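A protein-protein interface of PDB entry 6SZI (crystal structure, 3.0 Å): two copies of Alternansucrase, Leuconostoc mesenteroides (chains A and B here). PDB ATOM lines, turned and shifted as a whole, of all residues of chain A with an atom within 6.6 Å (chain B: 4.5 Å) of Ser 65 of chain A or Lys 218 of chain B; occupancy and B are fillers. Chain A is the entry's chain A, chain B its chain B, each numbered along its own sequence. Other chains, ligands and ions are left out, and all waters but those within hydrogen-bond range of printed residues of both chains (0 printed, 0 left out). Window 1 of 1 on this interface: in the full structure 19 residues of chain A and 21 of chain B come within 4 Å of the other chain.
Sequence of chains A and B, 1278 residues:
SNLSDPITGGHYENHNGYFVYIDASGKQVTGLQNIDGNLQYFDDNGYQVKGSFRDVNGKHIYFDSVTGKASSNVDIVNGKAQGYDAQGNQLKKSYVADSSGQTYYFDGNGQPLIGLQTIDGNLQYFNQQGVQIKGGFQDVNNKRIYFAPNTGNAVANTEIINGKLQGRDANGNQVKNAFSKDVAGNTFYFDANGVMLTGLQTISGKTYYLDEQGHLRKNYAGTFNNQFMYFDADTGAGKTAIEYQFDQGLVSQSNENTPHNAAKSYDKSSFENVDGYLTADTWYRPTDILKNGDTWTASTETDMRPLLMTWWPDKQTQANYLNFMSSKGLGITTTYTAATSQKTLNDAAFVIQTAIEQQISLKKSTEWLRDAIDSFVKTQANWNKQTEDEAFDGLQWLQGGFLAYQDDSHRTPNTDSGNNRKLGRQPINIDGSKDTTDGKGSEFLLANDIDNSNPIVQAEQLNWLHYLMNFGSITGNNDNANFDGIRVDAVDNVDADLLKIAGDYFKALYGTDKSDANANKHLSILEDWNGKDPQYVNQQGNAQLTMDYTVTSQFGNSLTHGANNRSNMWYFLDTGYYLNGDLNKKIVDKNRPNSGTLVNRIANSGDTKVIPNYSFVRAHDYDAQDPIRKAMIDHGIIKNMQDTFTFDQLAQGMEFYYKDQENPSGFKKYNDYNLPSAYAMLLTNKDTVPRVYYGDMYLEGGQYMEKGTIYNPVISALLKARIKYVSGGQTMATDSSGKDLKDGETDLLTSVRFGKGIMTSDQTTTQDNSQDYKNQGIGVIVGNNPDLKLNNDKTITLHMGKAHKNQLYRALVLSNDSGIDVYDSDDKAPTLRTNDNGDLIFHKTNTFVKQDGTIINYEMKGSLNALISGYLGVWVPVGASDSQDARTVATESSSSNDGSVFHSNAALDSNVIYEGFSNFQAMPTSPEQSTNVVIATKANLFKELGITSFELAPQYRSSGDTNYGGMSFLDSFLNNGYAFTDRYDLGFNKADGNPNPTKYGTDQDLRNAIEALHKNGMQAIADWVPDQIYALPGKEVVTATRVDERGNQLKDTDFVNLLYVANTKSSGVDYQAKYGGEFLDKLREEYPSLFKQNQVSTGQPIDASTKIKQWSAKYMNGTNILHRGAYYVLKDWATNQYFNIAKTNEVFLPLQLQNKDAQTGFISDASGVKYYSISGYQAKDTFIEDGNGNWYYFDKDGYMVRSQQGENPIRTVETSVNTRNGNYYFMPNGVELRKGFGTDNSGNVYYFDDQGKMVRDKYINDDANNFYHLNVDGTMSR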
ATOM      1  N   LYS A  50       7.690  23.888  15.473  1.00  0.00           N
ATOM      2  CA  LYS A  50       8.976  23.282  15.172  1.00  0.00           C
ATOM      3  C   LYS A  50       9.701  22.864  16.448  1.00  0.00           C
ATOM      4  O   LYS A  50       9.708  23.585  17.447  1.00  0.00           O
ATOM      5  CB  LYS A  50       9.845  24.265  14.411  1.00  0.00           C
ATOM      6  CG  LYS A  50       9.337  24.523  13.007  1.00  0.00           C
ATOM      7  CD  LYS A  50      10.306  25.360  12.180  1.00  0.00           C
ATOM      8  CE  LYS A  50       9.701  25.841  10.867  1.00  0.00           C
ATOM      9  NZ  LYS A  50      10.538  26.927  10.288  1.00  0.00           N
ATOM     10  N   GLY A  51      10.312  21.685  16.405  1.00  0.00           N
ATOM     11  CA  GLY A  51      11.067  21.146  17.541  1.00  0.00           C
ATOM     12  C   GLY A  51      10.258  20.901  18.819  1.00  0.00           C
ATOM     13  O   GLY A  51      10.801  20.899  19.921  1.00  0.00           O
ATOM     14  N   SER A  52       8.965  20.667  18.683  1.00  0.00           N
ATOM     15  CA  SER A  52       8.138  20.384  19.825  1.00  0.00           C
ATOM     16  C   SER A  52       7.197  19.224  19.471  1.00  0.00           C
ATOM     17  O   SER A  52       6.993  18.940  18.292  1.00  0.00           O
ATOM     18  CB  SER A  52       7.381  21.646  20.179  1.00  0.00           C
ATOM     19  OG  SER A  52       6.994  21.632  21.531  1.00  0.00           O
ATOM     20  N   TYR A  62       6.003  14.441  16.960  1.00  0.00           N
ATOM     21  CA  TYR A  62       7.070  15.454  16.998  1.00  0.00           C
ATOM     22  C   TYR A  62       7.202  16.088  15.635  1.00  0.00           C
ATOM     23  O   TYR A  62       6.971  15.438  14.626  1.00  0.00           O
ATOM     24  CB  TYR A  62       8.413  14.815  17.381  1.00  0.00           C
ATOM     25  CG  TYR A  62       9.607  15.767  17.437  1.00  0.00           C
ATOM     26  CD1 TYR A  62      10.655  15.656  16.520  1.00  0.00           C
ATOM     27  CD2 TYR A  62       9.701  16.761  18.419  1.00  0.00           C
ATOM     28  CE1 TYR A  62      11.754  16.514  16.565  1.00  0.00           C
ATOM     29  CE2 TYR A  62      10.797  17.623  18.469  1.00  0.00           C
ATOM     30  CZ  TYR A  62      11.820  17.499  17.537  1.00  0.00           C
ATOM     31  OH  TYR A  62      12.916  18.342  17.573  1.00  0.00           O
ATOM     32  N   PHE A  63       7.590  17.354  15.608  1.00  0.00           N
ATOM     33  CA  PHE A  63       7.844  18.057  14.357  1.00  0.00           C
ATOM     34  C   PHE A  63       9.283  18.607  14.396  1.00  0.00           C
ATOM     35  O   PHE A  63       9.779  18.998  15.459  1.00  0.00           O
ATOM     36  CB  PHE A  63       6.792  19.141  14.168  1.00  0.00           C
ATOM     37  CG  PHE A  63       5.369  18.619  14.148  1.00  0.00           C
ATOM     38  CD1 PHE A  63       4.709  18.399  12.954  1.00  0.00           C
ATOM     39  CD2 PHE A  63       4.689  18.351  15.319  1.00  0.00           C
ATOM     40  CE1 PHE A  63       3.399  17.931  12.927  1.00  0.00           C
ATOM     41  CE2 PHE A  63       3.382  17.873  15.295  1.00  0.00           C
ATOM     42  CZ  PHE A  63       2.738  17.666  14.097  1.00  0.00           C
ATOM     43  N   ASP A  64       9.963  18.593  13.248  1.00  0.00           N
ATOM     44  CA  ASP A  64      11.407  18.887  13.169  1.00  0.00           C
ATOM     45  C   ASP A  64      11.701  20.346  13.516  1.00  0.00           C
ATOM     46  O   ASP A  64      10.832  21.209  13.400  1.00  0.00           O
ATOM     47  CB  ASP A  64      11.954  18.557  11.770  1.00  0.00           C
ATOM     48  CG  ASP A  64      13.490  18.571  11.708  1.00  0.00           C
ATOM     49  OD1 ASP A  64      14.144  17.602  12.180  1.00  0.00           O
ATOM     50  OD2 ASP A  64      14.040  19.561  11.165  1.00  0.00           O
ATOM     51  N   SER A  65      12.927  20.607  13.967  1.00  0.00           N
ATOM     52  CA  SER A  65      13.317  21.934  14.423  1.00  0.00           C
ATOM     53  C   SER A  65      13.656  22.892  13.260  1.00  0.00           C
ATOM     54  O   SER A  65      13.527  24.109  13.418  1.00  0.00           O
ATOM     55  CB  SER A  65      14.499  21.823  15.396  1.00  0.00           C
ATOM     56  OG  SER A  65      15.732  21.790  14.708  1.00  0.00           O
ATOM     57  N   VAL A  66      14.093  22.358  12.112  1.00  0.00           N
ATOM     58  CA  VAL A  66      14.405  23.184  10.919  1.00  0.00           C
ATOM     59  C   VAL A  66      13.163  23.360  10.025  1.00  0.00           C
ATOM     60  O   VAL A  66      12.681  24.487   9.825  1.00  0.00           O
ATOM     61  CB  VAL A  66      15.579  22.591  10.087  1.00  0.00           C
ATOM     62  CG1 VAL A  66      15.780  23.355   8.784  1.00  0.00           C
ATOM     63  CG2 VAL A  66      16.871  22.607  10.892  1.00  0.00           C
ATOM     64  N   THR A  67      12.650  22.235   9.514  1.00  0.00           N
ATOM     65  CA  THR A  67      11.553  22.205   8.523  1.00  0.00           C
ATOM     66  C   THR A  67      10.136  22.214   9.141  1.00  0.00           C
ATOM     67  O   THR A  67       9.184  22.647   8.488  1.00  0.00           O
ATOM     68  CB  THR A  67      11.680  20.966   7.598  1.00  0.00           C
ATOM     69  OG1 THR A  67      11.523  19.765   8.365  1.00  0.00           O
ATOM     70  CG2 THR A  67      13.044  20.927   6.924  1.00  0.00           C
ATOM     71  N   GLY A  68      10.004  21.746  10.387  1.00  0.00           N
ATOM     72  CA  GLY A  68       8.692  21.616  11.059  1.00  0.00           C
ATOM     73  C   GLY A  68       7.896  20.414  10.592  1.00  0.00           C
ATOM     74  O   GLY A  68       6.674  20.360  10.759  1.00  0.00           O
ATOM     75  N   LYS A  69       8.618  19.454  10.014  1.00  0.00           N
ATOM     76  CA  LYS A  69       8.048  18.269   9.382  1.00  0.00           C
ATOM     77  C   LYS A  69       7.965  17.120  10.377  1.00  0.00           C
ATOM     78  O   LYS A  69       8.913  16.878  11.134  1.00  0.00           O
ATOM     79  CB  LYS A  69       8.934  17.842   8.203  1.00  0.00           C
ATOM     80  CG  LYS A  69       8.427  16.642   7.416  1.00  0.00           C
ATOM     81  CD  LYS A  69       9.505  16.042   6.529  1.00  0.00           C
ATOM     82  CE  LYS A  69       9.212  14.566   6.299  1.00  0.00           C
ATOM     83  NZ  LYS A  69      10.100  13.918   5.300  1.00  0.00           N
ATOM     84  N   SER A  99      16.270  13.794  19.176  1.00  0.00           N
ATOM     85  CA  SER A  99      16.753  15.048  18.587  1.00  0.00           C
ATOM     86  C   SER A  99      18.275  15.187  18.684  1.00  0.00           C
ATOM     87  O   SER A  99      18.908  15.627  17.730  1.00  0.00           O
ATOM     88  CB  SER A  99      16.074  16.251  19.249  1.00  0.00           C
ATOM     89  OG  SER A  99      14.695  16.305  18.898  1.00  0.00           O
ATOM     90  N   LEU B 216      25.450  26.457  15.761  1.00  0.00           N
ATOM     91  CA  LEU B 216      24.237  26.981  16.369  1.00  0.00           C
ATOM     92  C   LEU B 216      24.179  26.458  17.772  1.00  0.00           C
ATOM     93  O   LEU B 216      24.272  25.271  17.988  1.00  0.00           O
ATOM     94  CB  LEU B 216      23.014  26.503  15.603  1.00  0.00           C
ATOM     95  CG  LEU B 216      21.647  26.690  16.245  1.00  0.00           C
ATOM     96  CD1 LEU B 216      21.332  28.177  16.357  1.00  0.00           C
ATOM     97  CD2 LEU B 216      20.579  25.959  15.442  1.00  0.00           C
ATOM     98  N   ARG B 217      24.012  27.351  18.730  1.00  0.00           N
ATOM     99  CA  ARG B 217      24.012  26.976  20.142  1.00  0.00           C
ATOM    100  C   ARG B 217      22.587  26.887  20.689  1.00  0.00           C
ATOM    101  O   ARG B 217      21.825  27.847  20.599  1.00  0.00           O
ATOM    102  CB  ARG B 217      24.839  28.002  20.922  1.00  0.00           C
ATOM    103  CG  ARG B 217      26.205  28.257  20.290  1.00  0.00           C
ATOM    104  CD  ARG B 217      26.982  26.969  20.109  1.00  0.00           C
ATOM    105  NE  ARG B 217      27.072  26.301  21.394  1.00  0.00           N
ATOM    106  CZ  ARG B 217      28.142  26.329  22.173  1.00  0.00           C
ATOM    107  NH1 ARG B 217      29.259  26.943  21.782  1.00  0.00           N
ATOM    108  NH2 ARG B 217      28.111  25.707  23.340  1.00  0.00           N
ATOM    109  N   LYS B 218      22.235  25.729  21.222  1.00  0.00           N
ATOM    110  CA  LYS B 218      20.926  25.510  21.806  1.00  0.00           C
ATOM    111  C   LYS B 218      21.102  25.319  23.282  1.00  0.00           C
ATOM    112  O   LYS B 218      22.155  24.881  23.705  1.00  0.00           O
ATOM    113  CB  LYS B 218      20.278  24.274  21.210  1.00  0.00           C
ATOM    114  CG  LYS B 218      20.171  24.352  19.709  1.00  0.00           C
ATOM    115  CD  LYS B 218      19.424  23.164  19.149  1.00  0.00           C
ATOM    116  CE  LYS B 218      19.453  23.232  17.632  1.00  0.00           C
ATOM    117  NZ  LYS B 218      18.865  22.024  16.993  1.00  0.00           N
ATOM    118  N   ASN B 219      20.064  25.620  24.058  1.00  0.00           N
ATOM    119  CA  ASN B 219      20.118  25.559  25.514  1.00  0.00           C
ATOM    120  C   ASN B 219      21.341  26.325  26.040  1.00  0.00           C
ATOM    121  O   ASN B 219      22.208  25.765  26.748  1.00  0.00           O
ATOM    122  CB  ASN B 219      20.118  24.100  25.978  1.00  0.00           C
ATOM    123  CG  ASN B 219      19.880  23.953  27.462  1.00  0.00           C
ATOM    124  OD1 ASN B 219      19.033  24.638  28.033  1.00  0.00           O
ATOM    125  ND2 ASN B 219      20.638  23.054  28.107  1.00  0.00           N
ATOM    126  N   TYR B 220      21.389  27.604  25.660  1.00  0.00           N
ATOM    127  CA  TYR B 220      22.525  28.479  25.901  1.00  0.00           C
ATOM    128  C   TYR B 220      21.998  29.777  26.442  1.00  0.00           C
ATOM    129  O   TYR B 220      21.185  30.435  25.810  1.00  0.00           O
ATOM    130  CB  TYR B 220      23.289  28.744  24.591  1.00  0.00           C
ATOM    131  CG  TYR B 220      24.649  29.411  24.738  1.00  0.00           C
ATOM    132  CD1 TYR B 220      24.761  30.773  24.943  1.00  0.00           C
ATOM    133  CD2 TYR B 220      25.828  28.679  24.637  1.00  0.00           C
ATOM    134  CE1 TYR B 220      26.005  31.385  25.056  1.00  0.00           C
ATOM    135  CE2 TYR B 220      27.064  29.280  24.769  1.00  0.00           C
ATOM    136  CZ  TYR B 220      27.147  30.636  24.963  1.00  0.00           C
ATOM    137  OH  TYR B 220      28.361  31.256  25.080  1.00  0.00           O
ATOM    138  N   PHE B 231      18.707  30.880  24.628  1.00  0.00           N
ATOM    139  CA  PHE B 231      18.477  30.262  23.335  1.00  0.00           C
ATOM    140  C   PHE B 231      17.926  28.853  23.488  1.00  0.00           C
ATOM    141  O   PHE B 231      18.520  27.969  24.124  1.00  0.00           O
ATOM    142  CB  PHE B 231      19.743  30.286  22.525  1.00  0.00           C
ATOM    143  CG  PHE B 231      20.239  31.659  22.276  1.00  0.00           C
ATOM    144  CD1 PHE B 231      19.779  32.380  21.217  1.00  0.00           C
ATOM    145  CD2 PHE B 231      21.130  32.244  23.127  1.00  0.00           C
ATOM    146  CE1 PHE B 231      20.208  33.670  20.993  1.00  0.00           C
ATOM    147  CE2 PHE B 231      21.565  33.519  22.912  1.00  0.00           C
ATOM    148  CZ  PHE B 231      21.106  34.240  21.843  1.00  0.00           C
ATOM    149  N   ASP B 232      16.744  28.693  22.907  1.00  0.00           N
ATOM    150  CA  ASP B 232      15.887  27.511  23.002  1.00  0.00           C
ATOM    151  C   ASP B 232      16.631  26.180  22.935  1.00  0.00           C
ATOM    152  O   ASP B 232      17.573  26.051  22.158  1.00  0.00           O
ATOM    153  CB  ASP B 232      14.920  27.575  21.815  1.00  0.00           C
ATOM    154  CG  ASP B 232      13.598  26.982  22.106  1.00  0.00           C
ATOM    155  OD1 ASP B 232      13.539  25.966  22.827  1.00  0.00           O
ATOM    156  OD2 ASP B 232      12.617  27.567  21.603  1.00  0.00           O
ATOM    157  N   ALA B 233      16.208  25.192  23.721  1.00  0.00           N
ATOM    158  CA  ALA B 233      16.746  23.835  23.579  1.00  0.00           C
ATOM    159  C   ALA B 233      16.243  23.170  22.307  1.00  0.00           C
ATOM    160  O   ALA B 233      16.935  22.340  21.743  1.00  0.00           O
ATOM    161  CB  ALA B 233      16.401  22.993  24.785  1.00  0.00           C
ATOM    162  N   ASP B 234      15.051  23.549  21.849  1.00  0.00           N
ATOM    163  CA  ASP B 234      14.481  23.055  20.585  1.00  0.00           C
ATOM    164  C   ASP B 234      15.175  23.557  19.327  1.00  0.00           C
ATOM    165  O   ASP B 234      15.779  22.774  18.603  1.00  0.00           O
ATOM    166  CB  ASP B 234      12.997  23.432  20.464  1.00  0.00           C
ATOM    167  CG  ASP B 234      12.129  22.734  21.496  1.00  0.00           C
ATOM    168  OD1 ASP B 234      12.623  21.766  22.126  1.00  0.00           O
ATOM    169  OD2 ASP B 234      10.939  23.124  21.632  1.00  0.00           O
ATOM    170  N   THR B 235      15.053  24.848  19.046  1.00  0.00           N
ATOM    171  CA  THR B 235      15.523  25.422  17.776  1.00  0.00           C
ATOM    172  C   THR B 235      16.664  26.444  17.892  1.00  0.00           C
ATOM    173  O   THR B 235      17.200  26.906  16.887  1.00  0.00           O
ATOM    174  CB  THR B 235      14.370  26.122  17.055  1.00  0.00           C
ATOM    175  OG1 THR B 235      13.944  27.240  17.825  1.00  0.00           O
ATOM    176  CG2 THR B 235      13.198  25.182  16.878  1.00  0.00           C
ATOM    177  N   GLY B 236      17.056  26.767  19.121  1.00  0.00           N
ATOM    178  CA  GLY B 236      18.077  27.776  19.370  1.00  0.00           C
ATOM    179  C   GLY B 236      17.598  29.212  19.293  1.00  0.00           C
ATOM    180  O   GLY B 236      18.425  30.130  19.268  1.00  0.00           O
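N of Gly 51 of chain A lies within hydrogen-bond range of O of Phe 63 of chain A.
The side-chain carboxylate (OD1) of Asp 232 of chain B sits at hydrogen-bond distance from the backbone NH (N) of Asp 234 of chain B, at 3.0 Å.
The backbone NH (N) of Gly 51 of chain A lies within hydrogen-bond range of the backbone carbonyl oxygen (O) of Asp 64 of chain A (3.1 Å).
The side-chain amino group (NZ) of Lys 50 of chain A is in hydrogen-bond range of the backbone carbonyl oxygen (O) of Val 66 of chain A, 3.3 Å away.
No position is printed for both chains.
Of the 5 pairs that touch across the chains among the printed residues, none has its exchanged pair printed and touching as well.
Ser 65 of chain A touches three residues of chain B.
Lys 218 of chain B touches just one residue of chain A: Ser 65 (3.9 Å).
Printed residues of chain B within 4 Å of Gly 51 of chain A: Asp 234 (2.8 Å).
Of the printed residues of chain A, Asp 234 of chain B touches Gly 51 and Ser 65.
Of the 11 printed residues of chain B, 3 touch a printed residue of chain A.
Thr 235 of chain B touches Lys 50 of chain A.
Ser 65 of chain A touches Lys 218 of chain B (OG to NZ, 3.9 Å).
Asp 234 of chain B touches Ser 65 of chain A (O to CB, 3.6 Å).
Ser 65 of chain A touches Thr 235 of chain B (O to CG2, 3.6 Å).
The backbone carbonyl oxygen (O) of Gly 51 of chain A sits close to the side-chain carboxylate (OD2) of Asp 234 of chain B (2.8 Å).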
